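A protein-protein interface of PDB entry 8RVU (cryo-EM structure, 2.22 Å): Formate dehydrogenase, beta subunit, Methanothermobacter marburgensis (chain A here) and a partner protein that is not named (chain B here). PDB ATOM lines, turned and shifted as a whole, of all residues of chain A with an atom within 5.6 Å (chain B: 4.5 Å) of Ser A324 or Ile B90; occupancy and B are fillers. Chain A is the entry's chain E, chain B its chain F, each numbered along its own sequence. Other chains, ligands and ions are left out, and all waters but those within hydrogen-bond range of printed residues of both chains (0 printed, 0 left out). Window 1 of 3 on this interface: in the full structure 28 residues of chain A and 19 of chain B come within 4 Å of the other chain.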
ATOM      1  N   GLN A 319       9.891   3.402  -8.678  1.00  0.00           N
ATOM      2  CA  GLN A 319       8.564   3.598  -9.243  1.00  0.00           C
ATOM      3  C   GLN A 319       8.624   3.761 -10.754  1.00  0.00           C
ATOM      4  O   GLN A 319       7.799   3.186 -11.468  1.00  0.00           O
ATOM      5  CB  GLN A 319       7.888   4.810  -8.601  1.00  0.00           C
ATOM      6  CG  GLN A 319       7.859   4.786  -7.078  1.00  0.00           C
ATOM      7  CD  GLN A 319       6.876   3.768  -6.530  1.00  0.00           C
ATOM      8  OE1 GLN A 319       6.002   3.284  -7.248  1.00  0.00           O
ATOM      9  NE2 GLN A 319       7.013   3.443  -5.250  1.00  0.00           N
ATOM     10  N   GLY A 320       9.574   4.548 -11.267  1.00  0.00           N
ATOM     11  CA  GLY A 320       9.663   4.715 -12.705  1.00  0.00           C
ATOM     12  C   GLY A 320      10.061   3.431 -13.402  1.00  0.00           C
ATOM     13  O   GLY A 320       9.608   3.154 -14.512  1.00  0.00           O
ATOM     14  N   VAL A 321      10.914   2.629 -12.763  1.00  0.00           N
ATOM     15  CA  VAL A 321      11.281   1.341 -13.341  1.00  0.00           C
ATOM     16  C   VAL A 321      10.070   0.417 -13.393  1.00  0.00           C
ATOM     17  O   VAL A 321       9.790  -0.205 -14.424  1.00  0.00           O
ATOM     18  CB  VAL A 321      12.446   0.709 -12.557  1.00  0.00           C
ATOM     19  CG1 VAL A 321      12.716  -0.706 -13.058  1.00  0.00           C
ATOM     20  CG2 VAL A 321      13.691   1.564 -12.688  1.00  0.00           C
ATOM     21  N   ARG A 322       9.319   0.323 -12.289  1.00  0.00           N
ATOM     22  CA  ARG A 322       8.123  -0.514 -12.309  1.00  0.00           C
ATOM     23  C   ARG A 322       7.112   0.004 -13.328  1.00  0.00           C
ATOM     24  O   ARG A 322       6.423  -0.783 -13.993  1.00  0.00           O
ATOM     25  CB  ARG A 322       7.505  -0.583 -10.912  1.00  0.00           C
ATOM     26  CG  ARG A 322       6.415  -1.637 -10.774  1.00  0.00           C
ATOM     27  CD  ARG A 322       6.188  -2.049  -9.324  1.00  0.00           C
ATOM     28  NE  ARG A 322       5.054  -1.352  -8.727  1.00  0.00           N
ATOM     29  CZ  ARG A 322       3.784  -1.601  -9.016  1.00  0.00           C
ATOM     30  NH1 ARG A 322       3.441  -2.537  -9.886  1.00  0.00           N
ATOM     31  NH2 ARG A 322       2.832  -0.891  -8.418  1.00  0.00           N
ATOM     32  N   LEU A 323       7.006   1.330 -13.461  1.00  0.00           N
ATOM     33  CA  LEU A 323       6.120   1.918 -14.457  1.00  0.00           C
ATOM     34  C   LEU A 323       6.538   1.516 -15.864  1.00  0.00           C
ATOM     35  O   LEU A 323       5.733   0.982 -16.627  1.00  0.00           O
ATOM     36  CB  LEU A 323       6.110   3.440 -14.314  1.00  0.00           C
ATOM     37  CG  LEU A 323       5.256   4.003 -13.178  1.00  0.00           C
ATOM     38  CD1 LEU A 323       5.693   5.415 -12.837  1.00  0.00           C
ATOM     39  CD2 LEU A 323       3.784   3.970 -13.551  1.00  0.00           C
ATOM     40  N   SER A 324       7.805   1.719 -16.210  1.00  0.00           N
ATOM     41  CA  SER A 324       8.271   1.300 -17.523  1.00  0.00           C
ATOM     42  C   SER A 324       8.037  -0.185 -17.748  1.00  0.00           C
ATOM     43  O   SER A 324       7.801  -0.612 -18.883  1.00  0.00           O
ATOM     44  CB  SER A 324       9.751   1.628 -17.680  1.00  0.00           C
ATOM     45  OG  SER A 324      10.556   0.670 -17.020  1.00  0.00           O
ATOM     46  N   HIS A 325       8.096  -0.987 -16.683  1.00  0.00           N
ATOM     47  CA  HIS A 325       7.923  -2.427 -16.841  1.00  0.00           C
ATOM     48  C   HIS A 325       6.475  -2.802 -17.135  1.00  0.00           C
ATOM     49  O   HIS A 325       6.220  -3.635 -18.011  1.00  0.00           O
ATOM     50  CB  HIS A 325       8.409  -3.151 -15.587  1.00  0.00           C
ATOM     51  CG  HIS A 325       9.879  -3.429 -15.579  1.00  0.00           C
ATOM     52  ND1 HIS A 325      10.479  -4.226 -14.629  1.00  0.00           N
ATOM     53  CD2 HIS A 325      10.870  -3.014 -16.402  1.00  0.00           C
ATOM     54  CE1 HIS A 325      11.776  -4.292 -14.868  1.00  0.00           C
ATOM     55  NE2 HIS A 325      12.039  -3.566 -15.938  1.00  0.00           N
ATOM     56  N   MET A 326       5.512  -2.223 -16.407  1.00  0.00           N
ATOM     57  CA  MET A 326       4.145  -2.732 -16.496  1.00  0.00           C
ATOM     58  C   MET A 326       3.029  -1.692 -16.489  1.00  0.00           C
ATOM     59  O   MET A 326       1.860  -2.088 -16.510  1.00  0.00           O
ATOM     60  CB  MET A 326       3.886  -3.728 -15.348  1.00  0.00           C
ATOM     61  CG  MET A 326       4.380  -3.278 -13.976  1.00  0.00           C
ATOM     62  SD  MET A 326       3.541  -1.810 -13.344  1.00  0.00           S
ATOM     63  CE  MET A 326       1.855  -2.395 -13.224  1.00  0.00           C
ATOM     64  N   GLY A 327       3.327  -0.391 -16.477  1.00  0.00           N
ATOM     65  CA  GLY A 327       2.287   0.611 -16.336  1.00  0.00           C
ATOM     66  C   GLY A 327       1.356   0.699 -17.521  1.00  0.00           C
ATOM     67  O   GLY A 327       0.208   1.123 -17.359  1.00  0.00           O
ATOM     68  N   PHE A 328       1.823   0.320 -18.712  1.00  0.00           N
ATOM     69  CA  PHE A 328       0.914   0.167 -19.839  1.00  0.00           C
ATOM     70  C   PHE A 328      -0.111  -0.939 -19.651  1.00  0.00           C
ATOM     71  O   PHE A 328      -1.095  -0.988 -20.395  1.00  0.00           O
ATOM     72  CB  PHE A 328       1.694  -0.091 -21.132  1.00  0.00           C
ATOM     73  CG  PHE A 328       2.798  -1.103 -20.988  1.00  0.00           C
ATOM     74  CD1 PHE A 328       2.512  -2.455 -20.910  1.00  0.00           C
ATOM     75  CD2 PHE A 328       4.122  -0.701 -20.934  1.00  0.00           C
ATOM     76  CE1 PHE A 328       3.525  -3.385 -20.777  1.00  0.00           C
ATOM     77  CE2 PHE A 328       5.135  -1.627 -20.802  1.00  0.00           C
ATOM     78  CZ  PHE A 328       4.836  -2.968 -20.723  1.00  0.00           C
ATOM     79  N   ILE A 353      -0.533   7.081 -15.797  1.00  0.00           N
ATOM     80  CA  ILE A 353       0.394   6.660 -16.847  1.00  0.00           C
ATOM     81  C   ILE A 353      -0.296   5.704 -17.814  1.00  0.00           C
ATOM     82  O   ILE A 353      -0.157   5.820 -19.041  1.00  0.00           O
ATOM     83  CB  ILE A 353       1.651   6.025 -16.227  1.00  0.00           C
ATOM     84  CG1 ILE A 353       2.522   7.105 -15.580  1.00  0.00           C
ATOM     85  CG2 ILE A 353       2.417   5.218 -17.272  1.00  0.00           C
ATOM     86  CD1 ILE A 353       3.349   7.919 -16.562  1.00  0.00           C
ATOM     87  N   ALA B  47      13.818   1.700 -20.831  1.00  0.00           N
ATOM     88  CA  ALA B  47      13.606   2.828 -19.929  1.00  0.00           C
ATOM     89  C   ALA B  47      14.473   2.737 -18.682  1.00  0.00           C
ATOM     90  O   ALA B  47      14.758   3.762 -18.053  1.00  0.00           O
ATOM     91  CB  ALA B  47      12.138   2.902 -19.529  1.00  0.00           C
ATOM     92  N   PHE B  86       6.861   6.001 -24.484  1.00  0.00           N
ATOM     93  CA  PHE B  86       6.422   5.696 -23.124  1.00  0.00           C
ATOM     94  C   PHE B  86       7.306   6.393 -22.090  1.00  0.00           C
ATOM     95  O   PHE B  86       6.819   6.851 -21.049  1.00  0.00           O
ATOM     96  CB  PHE B  86       6.414   4.182 -22.899  1.00  0.00           C
ATOM     97  CG  PHE B  86       5.681   3.752 -21.655  1.00  0.00           C
ATOM     98  CD1 PHE B  86       4.502   4.371 -21.274  1.00  0.00           C
ATOM     99  CD2 PHE B  86       6.166   2.718 -20.871  1.00  0.00           C
ATOM    100  CE1 PHE B  86       3.829   3.976 -20.138  1.00  0.00           C
ATOM    101  CE2 PHE B  86       5.492   2.318 -19.732  1.00  0.00           C
ATOM    102  CZ  PHE B  86       4.323   2.950 -19.368  1.00  0.00           C
ATOM    103  N   ILE B  87       8.610   6.476 -22.357  1.00  0.00           N
ATOM    104  CA  ILE B  87       9.525   7.139 -21.429  1.00  0.00           C
ATOM    105  C   ILE B  87       9.219   8.629 -21.345  1.00  0.00           C
ATOM    106  O   ILE B  87       9.308   9.234 -20.270  1.00  0.00           O
ATOM    107  CB  ILE B  87      10.987   6.887 -21.842  1.00  0.00           C
ATOM    108  CG1 ILE B  87      11.362   5.421 -21.625  1.00  0.00           C
ATOM    109  CG2 ILE B  87      11.923   7.782 -21.052  1.00  0.00           C
ATOM    110  CD1 ILE B  87      12.500   4.948 -22.502  1.00  0.00           C
ATOM    111  N   GLU B  88       8.910   9.258 -22.481  1.00  0.00           N
ATOM    112  CA  GLU B  88       8.496  10.656 -22.437  1.00  0.00           C
ATOM    113  C   GLU B  88       7.217  10.819 -21.632  1.00  0.00           C
ATOM    114  O   GLU B  88       7.031  11.839 -20.960  1.00  0.00           O
ATOM    115  CB  GLU B  88       8.299  11.215 -23.843  1.00  0.00           C
ATOM    116  CG  GLU B  88       9.563  11.325 -24.664  1.00  0.00           C
ATOM    117  CD  GLU B  88       9.276  11.597 -26.125  1.00  0.00           C
ATOM    118  OE1 GLU B  88      10.172  12.119 -26.821  1.00  0.00           O
ATOM    119  OE2 GLU B  88       8.154  11.296 -26.580  1.00  0.00           O
ATOM    120  N   ASP B  89       6.318   9.837 -21.699  1.00  0.00           N
ATOM    121  CA  ASP B  89       5.151   9.870 -20.823  1.00  0.00           C
ATOM    122  C   ASP B  89       5.561   9.813 -19.354  1.00  0.00           C
ATOM    123  O   ASP B  89       5.050  10.576 -18.526  1.00  0.00           O
ATOM    124  CB  ASP B  89       4.205   8.714 -21.153  1.00  0.00           C
ATOM    125  CG  ASP B  89       3.244   9.044 -22.279  1.00  0.00           C
ATOM    126  OD1 ASP B  89       2.976  10.242 -22.509  1.00  0.00           O
ATOM    127  OD2 ASP B  89       2.752   8.102 -22.935  1.00  0.00           O
ATOM    128  N   ILE B  90       6.492   8.922 -19.014  1.00  0.00           N
ATOM    129  CA  ILE B  90       6.797   8.660 -17.608  1.00  0.00           C
ATOM    130  C   ILE B  90       7.602   9.796 -16.979  1.00  0.00           C
ATOM    131  O   ILE B  90       7.363  10.168 -15.825  1.00  0.00           O
ATOM    132  CB  ILE B  90       7.528   7.311 -17.465  1.00  0.00           C
ATOM    133  CG1 ILE B  90       6.529   6.158 -17.574  1.00  0.00           C
ATOM    134  CG2 ILE B  90       8.278   7.243 -16.140  1.00  0.00           C
ATOM    135  CD1 ILE B  90       7.168   4.818 -17.859  1.00  0.00           C
ATOM    136  N   LEU B  91       8.572  10.354 -17.703  1.00  0.00           N
ATOM    137  CA  LEU B  91       9.557  11.230 -17.069  1.00  0.00           C
ATOM    138  C   LEU B  91       8.949  12.450 -16.391  1.00  0.00           C
ATOM    139  O   LEU B  91       9.345  12.756 -15.253  1.00  0.00           O
ATOM    140  CB  LEU B  91      10.612  11.653 -18.097  1.00  0.00           C
ATOM    141  CG  LEU B  91      11.637  10.584 -18.480  1.00  0.00           C
ATOM    142  CD1 LEU B  91      12.360  10.966 -19.761  1.00  0.00           C
ATOM    143  CD2 LEU B  91      12.629  10.371 -17.348  1.00  0.00           C
ATOM    144  N   PRO B  92       8.018  13.188 -17.000  1.00  0.00           N
ATOM    145  CA  PRO B  92       7.522  14.413 -16.350  1.00  0.00           C
ATOM    146  C   PRO B  92       6.844  14.172 -15.012  1.00  0.00           C
ATOM    147  O   PRO B  92       6.727  15.113 -14.219  1.00  0.00           O
ATOM    148  CB  PRO B  92       6.539  14.985 -17.381  1.00  0.00           C
ATOM    149  CG  PRO B  92       6.956  14.389 -18.679  1.00  0.00           C
ATOM    150  CD  PRO B  92       7.454  13.019 -18.349  1.00  0.00           C
ATOM    151  N   GLU B  93       6.390  12.947 -14.733  1.00  0.00           N
ATOM    152  CA  GLU B  93       5.718  12.672 -13.468  1.00  0.00           C
ATOM    153  C   GLU B  93       6.658  12.765 -12.275  1.00  0.00           C
ATOM    154  O   GLU B  93       6.186  12.805 -11.134  1.00  0.00           O
ATOM    155  CB  GLU B  93       5.077  11.286 -13.503  1.00  0.00           C
ATOM    156  CG  GLU B  93       4.081  11.093 -14.625  1.00  0.00           C
ATOM    157  CD  GLU B  93       2.678  11.511 -14.242  1.00  0.00           C
ATOM    158  OE1 GLU B  93       2.524  12.571 -13.601  1.00  0.00           O
ATOM    159  OE2 GLU B  93       1.727  10.776 -14.580  1.00  0.00           O
ATOM    160  N   PHE B  94       7.970  12.789 -12.507  1.00  0.00           N
ATOM    161  CA  PHE B  94       8.954  12.892 -11.438  1.00  0.00           C
ATOM    162  C   PHE B  94       9.790  14.162 -11.543  1.00  0.00           C
ATOM    163  O   PHE B  94      10.911  14.206 -11.027  1.00  0.00           O
ATOM    164  CB  PHE B  94       9.851  11.655 -11.435  1.00  0.00           C
ATOM    165  CG  PHE B  94       9.101  10.373 -11.229  1.00  0.00           C
ATOM    166  CD1 PHE B  94       8.912   9.866  -9.955  1.00  0.00           C
ATOM    167  CD2 PHE B  94       8.576   9.679 -12.306  1.00  0.00           C
ATOM    168  CE1 PHE B  94       8.219   8.690  -9.757  1.00  0.00           C
ATOM    169  CE2 PHE B  94       7.881   8.503 -12.114  1.00  0.00           C
ATOM    170  CZ  PHE B  94       7.703   8.008 -10.838  1.00  0.00           C
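The side-chain hydroxyl (OG) of Ser A324 lies within hydrogen-bond range of the backbone carbonyl oxygen (O) of Val A321 (2.8 Å).
Of the printed residues of chain B, Leu A323 touches Phe B86 (3.4 Å), Ile B90 (3.9 Å) and Phe B94 (3.8 Å). Of chain B, only Ala B47, Phe B86 and Ile B90 come within 4 Å of Ser A324. Of the printed residues of chain B, Phe A328 touches Phe B86. Of the printed residues of chain B, Ile A353 touches Phe B86, Asp B89, Ile B90 and Glu B93. Of the printed residues of chain A, Phe B86 touches Leu A323 (3.4 Å), Ser A324 (3.7 Å), Phe A328 (3.5 Å) and Ile A353 (3.4 Å). Of chain A, only Leu A323, Ser A324 and Ile A353 come within 4 Å of Ile B90. The nearest printed residue of chain A that does not touch Asp B89 is Leu A323 (7.7 Å).
Printed residues of chain B that touch a printed residue of chain A: Ala B47, Phe B86, Asp B89, Ile B90, Glu B93 and Phe B94. Of the 11 printed residues of chain A, 6 touch a printed residue of chain B. Hydrophobic or aromatic side chains of chain A within 4 Å of the printed part of chain B: Leu A323, Phe A328 and Ile A353. Along chain A the printed residues that touch a printed residue of chain B span positions 319 to 353. Among the printed residues, 13 pairs touch across the chains. Among the printed residues, no Asp or Glu carboxylate lies within 4 Å of a Lys or Arg side-chain nitrogen of the other chain.
Among the printed residues, pairs that only touch across the chains: Ser A324 with Ala B47 (3.3 Å), Leu A323 with Phe B86 (3.4 Å), Ile A353 with Phe B86 (3.4 Å), Phe A328 with Phe B86 (3.5 Å), Ser A324 with Ile B90 (3.6 Å), Ile A353 with Ile B90 (3.7 Å), Ser A324 with Phe B86 (3.7 Å), Ile A353 with Asp B89 (3.7 Å), Ile A353 with Glu B93 (3.8 Å), Leu A323 with Phe B94 (3.8 Å), Gln A319 with Phe B94 (3.9 Å), Leu A323 with Ile B90 (3.9 Å) and Gly A320 with Phe B94 (3.96 Å).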
